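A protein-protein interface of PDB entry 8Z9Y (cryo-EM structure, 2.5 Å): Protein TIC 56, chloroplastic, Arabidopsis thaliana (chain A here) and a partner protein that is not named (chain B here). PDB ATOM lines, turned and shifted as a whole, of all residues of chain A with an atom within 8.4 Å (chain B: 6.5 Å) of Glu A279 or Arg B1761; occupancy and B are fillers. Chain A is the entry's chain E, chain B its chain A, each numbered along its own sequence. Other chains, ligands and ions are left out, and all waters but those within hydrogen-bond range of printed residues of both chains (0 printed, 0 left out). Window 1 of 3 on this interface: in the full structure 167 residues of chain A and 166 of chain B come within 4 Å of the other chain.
The side-chain carboxylate of Glu A279 lies within salt-bridge range of the guanidinium group of Arg B1761 (3.1 Å).
The side-chain hydroxyl of Tyr B1762 sits at hydrogen-bond distance from the backbone carbonyl oxygen of Ile B1777, at 3.1 Å.
A ring nitrogen (ND1) of His B1771 lies within hydrogen-bond range of the backbone carbonyl oxygen of Asn B1765 (2.9 Å).
The backbone NH of Ile A272 sits at hydrogen-bond distance from the backbone carbonyl oxygen of Ala A281, at 2.8 Å.
Among the printed residues, merely in contact across the chains: Ala A281 with Ile B1777 (3.7 Å), Asp A278 with His B1771 (3.8 Å) and Met A285 with Ile B1777 (3.8 Å).
Of chain B, only Arg B1761 (3.1 Å) comes within 4 Å of Glu A279.
Of the printed residues of chain B, Asp A278 touches His B1771 (3.8 Å).
Of the printed residues of chain B, Ala A281 touches Ile B1777.
The nearest printed residue of chain A that does not touch His B1771 is Glu A279 (4.9 Å).
Of the 14 printed residues of chain A, 4 touch a printed residue of chain B.
Printed residues of chain A that touch a printed residue of chain B: Asp A278, Glu A279, Ala A281 and Met A285.
Hydrophobic or aromatic side chains of chain A that line the printed part of chain B: Ala A281 and Met A285.
Along chain A the printed residues that touch a printed residue of chain B span positions 278 to 285.
Of the 15 printed residues of chain B, 3 touch a printed residue of chain A.
Printed residues of chain B that touch a printed residue of chain A: Arg B1761, His B1771 and Ile B1777.
Hydrophobic or aromatic side chains of chain B that line the printed part of chain A: Ile B1777.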
ATOM      1  N   PHE A 271      10.718 -22.639 -14.889  1.00  0.00           N
ATOM      2  CA  PHE A 271       9.785 -23.613 -14.342  1.00  0.00           C
ATOM      3  C   PHE A 271      10.545 -24.837 -13.847  1.00  0.00           C
ATOM      4  O   PHE A 271      11.390 -25.384 -14.560  1.00  0.00           O
ATOM      5  CB  PHE A 271       8.756 -24.013 -15.398  1.00  0.00           C
ATOM      6  CG  PHE A 271       7.561 -23.110 -15.447  1.00  0.00           C
ATOM      7  CD1 PHE A 271       7.683 -21.802 -15.879  1.00  0.00           C
ATOM      8  CD2 PHE A 271       6.313 -23.567 -15.060  1.00  0.00           C
ATOM      9  CE1 PHE A 271       6.587 -20.966 -15.924  1.00  0.00           C
ATOM     10  CE2 PHE A 271       5.213 -22.736 -15.104  1.00  0.00           C
ATOM     11  CZ  PHE A 271       5.350 -21.434 -15.536  1.00  0.00           C
ATOM     12  N   ILE A 272      10.239 -25.265 -12.623  1.00  0.00           N
ATOM     13  CA  ILE A 272      10.960 -26.342 -11.961  1.00  0.00           C
ATOM     14  C   ILE A 272       9.953 -27.318 -11.371  1.00  0.00           C
ATOM     15  O   ILE A 272       8.801 -26.974 -11.099  1.00  0.00           O
ATOM     16  CB  ILE A 272      11.910 -25.802 -10.866  1.00  0.00           C
ATOM     17  CG1 ILE A 272      12.981 -26.831 -10.508  1.00  0.00           C
ATOM     18  CG2 ILE A 272      11.128 -25.400  -9.628  1.00  0.00           C
ATOM     19  CD1 ILE A 272      14.285 -26.215 -10.063  1.00  0.00           C
ATOM     20  N   TRP A 273      10.397 -28.560 -11.187  1.00  0.00           N
ATOM     21  CA  TRP A 273       9.603 -29.581 -10.519  1.00  0.00           C
ATOM     22  C   TRP A 273      10.432 -30.243  -9.431  1.00  0.00           C
ATOM     23  O   TRP A 273      11.590 -30.607  -9.655  1.00  0.00           O
ATOM     24  CB  TRP A 273       9.095 -30.645 -11.493  1.00  0.00           C
ATOM     25  CG  TRP A 273       8.168 -31.609 -10.829  1.00  0.00           C
ATOM     26  CD1 TRP A 273       6.832 -31.445 -10.615  1.00  0.00           C
ATOM     27  CD2 TRP A 273       8.512 -32.878 -10.261  1.00  0.00           C
ATOM     28  NE1 TRP A 273       6.320 -32.537  -9.962  1.00  0.00           N
ATOM     29  CE2 TRP A 273       7.332 -33.431  -9.732  1.00  0.00           C
ATOM     30  CE3 TRP A 273       9.704 -33.601 -10.155  1.00  0.00           C
ATOM     31  CZ2 TRP A 273       7.307 -34.674  -9.105  1.00  0.00           C
ATOM     32  CZ3 TRP A 273       9.677 -34.835  -9.532  1.00  0.00           C
ATOM     33  CH2 TRP A 273       8.487 -35.357  -9.012  1.00  0.00           C
ATOM     34  N   GLY A 274       9.827 -30.408  -8.259  1.00  0.00           N
ATOM     35  CA  GLY A 274      10.517 -30.970  -7.116  1.00  0.00           C
ATOM     36  C   GLY A 274       9.860 -32.222  -6.579  1.00  0.00           C
ATOM     37  O   GLY A 274       9.031 -32.832  -7.257  1.00  0.00           O
ATOM     38  N   GLU A 275      10.209 -32.607  -5.352  1.00  0.00           N
ATOM     39  CA  GLU A 275       9.753 -33.886  -4.818  1.00  0.00           C
ATOM     40  C   GLU A 275       8.251 -33.879  -4.559  1.00  0.00           C
ATOM     41  O   GLU A 275       7.503 -34.661  -5.154  1.00  0.00           O
ATOM     42  CB  GLU A 275      10.519 -34.220  -3.537  1.00  0.00           C
ATOM     43  CG  GLU A 275      10.345 -35.649  -3.019  1.00  0.00           C
ATOM     44  CD  GLU A 275      10.717 -36.720  -4.035  1.00  0.00           C
ATOM     45  OE1 GLU A 275       9.979 -36.908  -5.025  1.00  0.00           O
ATOM     46  OE2 GLU A 275      11.760 -37.379  -3.838  1.00  0.00           O
ATOM     47  N   ASP A 276       7.787 -32.991  -3.681  1.00  0.00           N
ATOM     48  CA  ASP A 276       6.426 -33.054  -3.164  1.00  0.00           C
ATOM     49  C   ASP A 276       5.515 -31.974  -3.740  1.00  0.00           C
ATOM     50  O   ASP A 276       4.556 -31.562  -3.079  1.00  0.00           O
ATOM     51  CB  ASP A 276       6.441 -32.972  -1.639  1.00  0.00           C
ATOM     52  CG  ASP A 276       5.479 -33.946  -0.996  1.00  0.00           C
ATOM     53  OD1 ASP A 276       5.279 -35.041  -1.561  1.00  0.00           O
ATOM     54  OD2 ASP A 276       4.925 -33.621   0.074  1.00  0.00           O
ATOM     55  N   MET A 277       5.785 -31.505  -4.954  1.00  0.00           N
ATOM     56  CA  MET A 277       4.910 -30.550  -5.616  1.00  0.00           C
ATOM     57  C   MET A 277       4.063 -31.254  -6.667  1.00  0.00           C
ATOM     58  O   MET A 277       4.454 -32.286  -7.218  1.00  0.00           O
ATOM     59  CB  MET A 277       5.699 -29.406  -6.258  1.00  0.00           C
ATOM     60  CG  MET A 277       6.727 -28.770  -5.343  1.00  0.00           C
ATOM     61  SD  MET A 277       7.516 -27.329  -6.084  1.00  0.00           S
ATOM     62  CE  MET A 277       7.786 -27.908  -7.753  1.00  0.00           C
ATOM     63  N   ASP A 278       2.891 -30.681  -6.935  1.00  0.00           N
ATOM     64  CA  ASP A 278       1.916 -31.288  -7.827  1.00  0.00           C
ATOM     65  C   ASP A 278       2.054 -30.829  -9.272  1.00  0.00           C
ATOM     66  O   ASP A 278       1.627 -31.552 -10.180  1.00  0.00           O
ATOM     67  CB  ASP A 278       0.500 -30.982  -7.331  1.00  0.00           C
ATOM     68  CG  ASP A 278      -0.561 -31.736  -8.098  1.00  0.00           C
ATOM     69  OD1 ASP A 278      -0.281 -32.873  -8.530  1.00  0.00           O
ATOM     70  OD2 ASP A 278      -1.673 -31.194  -8.267  1.00  0.00           O
ATOM     71  N   GLU A 279       2.639 -29.659  -9.511  1.00  0.00           N
ATOM     72  CA  GLU A 279       2.754 -29.128 -10.859  1.00  0.00           C
ATOM     73  C   GLU A 279       4.009 -28.275 -10.954  1.00  0.00           C
ATOM     74  O   GLU A 279       4.572 -27.849  -9.943  1.00  0.00           O
ATOM     75  CB  GLU A 279       1.520 -28.307 -11.247  1.00  0.00           C
ATOM     76  CG  GLU A 279       1.306 -27.075 -10.384  1.00  0.00           C
ATOM     77  CD  GLU A 279       0.039 -26.325 -10.740  1.00  0.00           C
ATOM     78  OE1 GLU A 279      -1.055 -26.918 -10.630  1.00  0.00           O
ATOM     79  OE2 GLU A 279       0.135 -25.143 -11.130  1.00  0.00           O
ATOM     80  N   TRP A 280       4.443 -28.037 -12.187  1.00  0.00           N
ATOM     81  CA  TRP A 280       5.622 -27.216 -12.419  1.00  0.00           C
ATOM     82  C   TRP A 280       5.329 -25.762 -12.077  1.00  0.00           C
ATOM     83  O   TRP A 280       4.251 -25.243 -12.373  1.00  0.00           O
ATOM     84  CB  TRP A 280       6.073 -27.340 -13.873  1.00  0.00           C
ATOM     85  CG  TRP A 280       6.448 -28.736 -14.264  1.00  0.00           C
ATOM     86  CD1 TRP A 280       5.620 -29.816 -14.341  1.00  0.00           C
ATOM     87  CD2 TRP A 280       7.751 -29.203 -14.628  1.00  0.00           C
ATOM     88  NE1 TRP A 280       6.325 -30.927 -14.731  1.00  0.00           N
ATOM     89  CE2 TRP A 280       7.636 -30.577 -14.914  1.00  0.00           C
ATOM     90  CE3 TRP A 280       9.003 -28.594 -14.741  1.00  0.00           C
ATOM     91  CZ2 TRP A 280       8.724 -31.351 -15.305  1.00  0.00           C
ATOM     92  CZ3 TRP A 280      10.081 -29.363 -15.129  1.00  0.00           C
ATOM     93  CH2 TRP A 280       9.936 -30.726 -15.407  1.00  0.00           C
ATOM     94  N   ALA A 281       6.295 -25.105 -11.446  1.00  0.00           N
ATOM     95  CA  ALA A 281       6.115 -23.742 -10.974  1.00  0.00           C
ATOM     96  C   ALA A 281       7.435 -23.003 -11.112  1.00  0.00           C
ATOM     97  O   ALA A 281       8.501 -23.629 -11.142  1.00  0.00           O
ATOM     98  CB  ALA A 281       5.637 -23.716  -9.516  1.00  0.00           C
ATOM     99  N   PRO A 282       7.401 -21.676 -11.204  1.00  0.00           N
ATOM    100  CA  PRO A 282       8.649 -20.907 -11.228  1.00  0.00           C
ATOM    101  C   PRO A 282       9.403 -21.028  -9.913  1.00  0.00           C
ATOM    102  O   PRO A 282       8.832 -21.303  -8.855  1.00  0.00           O
ATOM    103  CB  PRO A 282       8.183 -19.467 -11.467  1.00  0.00           C
ATOM    104  CG  PRO A 282       6.809 -19.588 -12.020  1.00  0.00           C
ATOM    105  CD  PRO A 282       6.223 -20.821 -11.417  1.00  0.00           C
ATOM    106  N   MET A 285       8.330 -18.663  -7.029  1.00  0.00           N
ATOM    107  CA  MET A 285       7.066 -18.918  -6.347  1.00  0.00           C
ATOM    108  C   MET A 285       7.174 -20.017  -5.295  1.00  0.00           C
ATOM    109  O   MET A 285       6.402 -20.016  -4.331  1.00  0.00           O
ATOM    110  CB  MET A 285       5.986 -19.278  -7.367  1.00  0.00           C
ATOM    111  CG  MET A 285       5.721 -18.188  -8.388  1.00  0.00           C
ATOM    112  SD  MET A 285       5.795 -16.535  -7.676  1.00  0.00           S
ATOM    113  CE  MET A 285       4.131 -16.364  -7.046  1.00  0.00           C
ATOM    114  N   VAL A 286       8.106 -20.956  -5.456  1.00  0.00           N
ATOM    115  CA  VAL A 286       8.197 -22.087  -4.541  1.00  0.00           C
ATOM    116  C   VAL A 286       8.705 -21.615  -3.185  1.00  0.00           C
ATOM    117  O   VAL A 286       9.661 -20.834  -3.098  1.00  0.00           O
ATOM    118  CB  VAL A 286       9.100 -23.183  -5.125  1.00  0.00           C
ATOM    119  CG1 VAL A 286       9.083 -24.415  -4.237  1.00  0.00           C
ATOM    120  CG2 VAL A 286       8.649 -23.539  -6.529  1.00  0.00           C
ATOM    121  N   LEU B1756      -7.488 -19.016 -16.319  1.00  0.00           N
ATOM    122  CA  LEU B1756      -7.909 -20.388 -16.067  1.00  0.00           C
ATOM    123  C   LEU B1756      -6.850 -21.161 -15.296  1.00  0.00           C
ATOM    124  O   LEU B1756      -7.184 -21.990 -14.445  1.00  0.00           O
ATOM    125  CB  LEU B1756      -8.235 -21.086 -17.386  1.00  0.00           C
ATOM    126  CG  LEU B1756      -9.591 -20.744 -18.002  1.00  0.00           C
ATOM    127  CD1 LEU B1756      -9.812 -21.531 -19.279  1.00  0.00           C
ATOM    128  CD2 LEU B1756     -10.702 -21.025 -17.008  1.00  0.00           C
ATOM    129  N   ALA B1757      -5.569 -20.912 -15.580  1.00  0.00           N
ATOM    130  CA  ALA B1757      -4.516 -21.563 -14.810  1.00  0.00           C
ATOM    131  C   ALA B1757      -4.575 -21.150 -13.346  1.00  0.00           C
ATOM    132  O   ALA B1757      -4.462 -21.993 -12.448  1.00  0.00           O
ATOM    133  CB  ALA B1757      -3.149 -21.239 -15.411  1.00  0.00           C
ATOM    134  N   CYS B1758      -4.772 -19.855 -13.084  1.00  0.00           N
ATOM    135  CA  CYS B1758      -4.885 -19.400 -11.700  1.00  0.00           C
ATOM    136  C   CYS B1758      -6.097 -20.018 -11.010  1.00  0.00           C
ATOM    137  O   CYS B1758      -6.009 -20.453  -9.854  1.00  0.00           O
ATOM    138  CB  CYS B1758      -4.960 -17.875 -11.653  1.00  0.00           C
ATOM    139  SG  CYS B1758      -4.647 -17.170 -10.020  1.00  0.00           S
ATOM    140  N   MET B1759      -7.237 -20.068 -11.706  1.00  0.00           N
ATOM    141  CA  MET B1759      -8.435 -20.664 -11.117  1.00  0.00           C
ATOM    142  C   MET B1759      -8.230 -22.144 -10.821  1.00  0.00           C
ATOM    143  O   MET B1759      -8.640 -22.634  -9.764  1.00  0.00           O
ATOM    144  CB  MET B1759      -9.637 -20.466 -12.039  1.00  0.00           C
ATOM    145  CG  MET B1759      -9.978 -19.016 -12.323  1.00  0.00           C
ATOM    146  SD  MET B1759     -11.724 -18.769 -12.688  1.00  0.00           S
ATOM    147  CE  MET B1759     -11.889 -17.018 -12.356  1.00  0.00           C
ATOM    148  N   ASN B1760      -7.599 -22.873 -11.741  1.00  0.00           N
ATOM    149  CA  ASN B1760      -7.326 -24.283 -11.496  1.00  0.00           C
ATOM    150  C   ASN B1760      -6.379 -24.458 -10.317  1.00  0.00           C
ATOM    151  O   ASN B1760      -6.489 -25.430  -9.561  1.00  0.00           O
ATOM    152  CB  ASN B1760      -6.747 -24.933 -12.751  1.00  0.00           C
ATOM    153  CG  ASN B1760      -6.983 -26.426 -12.791  1.00  0.00           C
ATOM    154  OD1 ASN B1760      -8.041 -26.910 -12.390  1.00  0.00           O
ATOM    155  ND2 ASN B1760      -5.996 -27.168 -13.276  1.00  0.00           N
ATOM    156  N   ARG B1761      -5.438 -23.528 -10.149  1.00  0.00           N
ATOM    157  CA  ARG B1761      -4.527 -23.603  -9.013  1.00  0.00           C
ATOM    158  C   ARG B1761      -5.260 -23.392  -7.692  1.00  0.00           C
ATOM    159  O   ARG B1761      -5.063 -24.153  -6.737  1.00  0.00           O
ATOM    160  CB  ARG B1761      -3.406 -22.572  -9.160  1.00  0.00           C
ATOM    161  CG  ARG B1761      -2.460 -22.846 -10.317  1.00  0.00           C
ATOM    162  CD  ARG B1761      -1.317 -21.849 -10.434  1.00  0.00           C
ATOM    163  NE  ARG B1761      -0.477 -22.113 -11.599  1.00  0.00           N
ATOM    164  CZ  ARG B1761       0.514 -21.328 -11.996  1.00  0.00           C
ATOM    165  NH1 ARG B1761       0.799 -20.223 -11.319  1.00  0.00           N
ATOM    166  NH2 ARG B1761       1.227 -21.646 -13.068  1.00  0.00           N
ATOM    167  N   TYR B1762      -6.113 -22.368  -7.615  1.00  0.00           N
ATOM    168  CA  TYR B1762      -6.577 -21.886  -6.320  1.00  0.00           C
ATOM    169  C   TYR B1762      -8.087 -21.866  -6.118  1.00  0.00           C
ATOM    170  O   TYR B1762      -8.534 -21.467  -5.037  1.00  0.00           O
ATOM    171  CB  TYR B1762      -6.035 -20.472  -6.066  1.00  0.00           C
ATOM    172  CG  TYR B1762      -4.575 -20.435  -5.683  1.00  0.00           C
ATOM    173  CD1 TYR B1762      -4.151 -20.897  -4.447  1.00  0.00           C
ATOM    174  CD2 TYR B1762      -3.622 -19.935  -6.558  1.00  0.00           C
ATOM    175  CE1 TYR B1762      -2.818 -20.865  -4.092  1.00  0.00           C
ATOM    176  CE2 TYR B1762      -2.287 -19.899  -6.213  1.00  0.00           C
ATOM    177  CZ  TYR B1762      -1.891 -20.364  -4.979  1.00  0.00           C
ATOM    178  OH  TYR B1762      -0.562 -20.329  -4.630  1.00  0.00           O
ATOM    179  N   TRP B1763      -8.893 -22.274  -7.099  1.00  0.00           N
ATOM    180  CA  TRP B1763     -10.333 -22.086  -6.980  1.00  0.00           C
ATOM    181  C   TRP B1763     -11.143 -23.371  -6.894  1.00  0.00           C
ATOM    182  O   TRP B1763     -12.301 -23.315  -6.473  1.00  0.00           O
ATOM    183  CB  TRP B1763     -10.864 -21.251  -8.156  1.00  0.00           C
ATOM    184  CG  TRP B1763     -10.581 -19.789  -8.021  1.00  0.00           C
ATOM    185  CD1 TRP B1763      -9.388 -19.213  -7.702  1.00  0.00           C
ATOM    186  CD2 TRP B1763     -11.509 -18.715  -8.202  1.00  0.00           C
ATOM    187  NE1 TRP B1763      -9.514 -17.847  -7.672  1.00  0.00           N
ATOM    188  CE2 TRP B1763     -10.807 -17.516  -7.977  1.00  0.00           C
ATOM    189  CE3 TRP B1763     -12.863 -18.651  -8.535  1.00  0.00           C
ATOM    190  CZ2 TRP B1763     -11.414 -16.268  -8.073  1.00  0.00           C
ATOM    191  CZ3 TRP B1763     -13.464 -17.410  -8.628  1.00  0.00           C
ATOM    192  CH2 TRP B1763     -12.741 -16.236  -8.399  1.00  0.00           C
ATOM    193  N   PHE B1764     -10.585 -24.517  -7.276  1.00  0.00           N
ATOM    194  CA  PHE B1764     -11.339 -25.763  -7.292  1.00  0.00           C
ATOM    195  C   PHE B1764     -10.523 -26.894  -6.686  1.00  0.00           C
ATOM    196  O   PHE B1764      -9.333 -27.041  -6.982  1.00  0.00           O
ATOM    197  CB  PHE B1764     -11.757 -26.139  -8.716  1.00  0.00           C
ATOM    198  CG  PHE B1764     -12.913 -25.338  -9.238  1.00  0.00           C
ATOM    199  CD1 PHE B1764     -14.213 -25.729  -8.981  1.00  0.00           C
ATOM    200  CD2 PHE B1764     -12.698 -24.193  -9.985  1.00  0.00           C
ATOM    201  CE1 PHE B1764     -15.279 -24.996  -9.458  1.00  0.00           C
ATOM    202  CE2 PHE B1764     -13.760 -23.455 -10.464  1.00  0.00           C
ATOM    203  CZ  PHE B1764     -15.052 -23.857 -10.201  1.00  0.00           C
ATOM    204  N   ASN B1765     -11.180 -27.696  -5.844  1.00  0.00           N
ATOM    205  CA  ASN B1765     -10.589 -28.902  -5.262  1.00  0.00           C
ATOM    206  C   ASN B1765      -9.262 -28.598  -4.571  1.00  0.00           C
ATOM    207  O   ASN B1765      -8.295 -29.355  -4.671  1.00  0.00           O
ATOM    208  CB  ASN B1765     -10.413 -29.989  -6.323  1.00  0.00           C
ATOM    209  CG  ASN B1765     -11.732 -30.452  -6.905  1.00  0.00           C
ATOM    210  OD1 ASN B1765     -12.615 -30.913  -6.183  1.00  0.00           O
ATOM    211  ND2 ASN B1765     -11.873 -30.332  -8.219  1.00  0.00           N
ATOM    212  N   THR B1766      -9.217 -27.475  -3.862  1.00  0.00           N
ATOM    213  CA  THR B1766      -7.986 -27.007  -3.243  1.00  0.00           C
ATOM    214  C   THR B1766      -7.718 -27.623  -1.876  1.00  0.00           C
ATOM    215  O   THR B1766      -6.644 -27.388  -1.314  1.00  0.00           O
ATOM    216  CB  THR B1766      -8.013 -25.480  -3.114  1.00  0.00           C
ATOM    217  OG1 THR B1766      -6.737 -25.014  -2.665  1.00  0.00           O
ATOM    218  CG2 THR B1766      -9.082 -25.047  -2.127  1.00  0.00           C
ATOM    219  N   HIS B1771      -4.420 -31.078  -4.844  1.00  0.00           N
ATOM    220  CA  HIS B1771      -3.472 -30.009  -5.116  1.00  0.00           C
ATOM    221  C   HIS B1771      -2.613 -29.744  -3.888  1.00  0.00           C
ATOM    222  O   HIS B1771      -3.101 -29.795  -2.755  1.00  0.00           O
ATOM    223  CB  HIS B1771      -4.191 -28.720  -5.528  1.00  0.00           C
ATOM    224  CG  HIS B1771      -5.038 -28.865  -6.755  1.00  0.00           C
ATOM    225  ND1 HIS B1771      -6.232 -29.553  -6.758  1.00  0.00           N
ATOM    226  CD2 HIS B1771      -4.863 -28.409  -8.016  1.00  0.00           C
ATOM    227  CE1 HIS B1771      -6.756 -29.514  -7.970  1.00  0.00           C
ATOM    228  NE2 HIS B1771      -5.944 -28.827  -8.753  1.00  0.00           N
ATOM    229  N   SER B1773      -0.770 -26.817  -3.963  1.00  0.00           N
ATOM    230  CA  SER B1773      -0.370 -25.441  -4.238  1.00  0.00           C
ATOM    231  C   SER B1773      -0.510 -24.541  -3.018  1.00  0.00           C
ATOM    232  O   SER B1773       0.257 -23.584  -2.868  1.00  0.00           O
ATOM    233  CB  SER B1773      -1.192 -24.883  -5.398  1.00  0.00           C
ATOM    234  OG  SER B1773      -1.060 -25.696  -6.551  1.00  0.00           O
ATOM    235  N   MET B1774      -1.477 -24.821  -2.143  1.00  0.00           N
ATOM    236  CA  MET B1774      -1.719 -23.931  -1.012  1.00  0.00           C
ATOM    237  C   MET B1774      -0.565 -23.957  -0.019  1.00  0.00           C
ATOM    238  O   MET B1774      -0.260 -22.940   0.614  1.00  0.00           O
ATOM    239  CB  MET B1774      -3.027 -24.301  -0.318  1.00  0.00           C
ATOM    240  CG  MET B1774      -4.263 -23.799  -1.032  1.00  0.00           C
ATOM    241  SD  MET B1774      -4.804 -22.219  -0.363  1.00  0.00           S
ATOM    242  CE  MET B1774      -5.172 -22.695   1.318  1.00  0.00           C
ATOM    243  N   ILE B1777       3.193 -23.412  -2.881  1.00  0.00           N
ATOM    244  CA  ILE B1777       3.340 -22.281  -3.789  1.00  0.00           C
ATOM    245  C   ILE B1777       2.825 -21.026  -3.101  1.00  0.00           C
ATOM    246  O   ILE B1777       1.705 -21.015  -2.575  1.00  0.00           O
ATOM    247  CB  ILE B1777       2.598 -22.523  -5.114  1.00  0.00           C
ATOM    248  CG1 ILE B1777       2.927 -23.911  -5.661  1.00  0.00           C
ATOM    249  CG2 ILE B1777       2.957 -21.452  -6.126  1.00  0.00           C
ATOM    250  CD1 ILE B1777       4.382 -24.094  -6.019  1.00  0.00           C
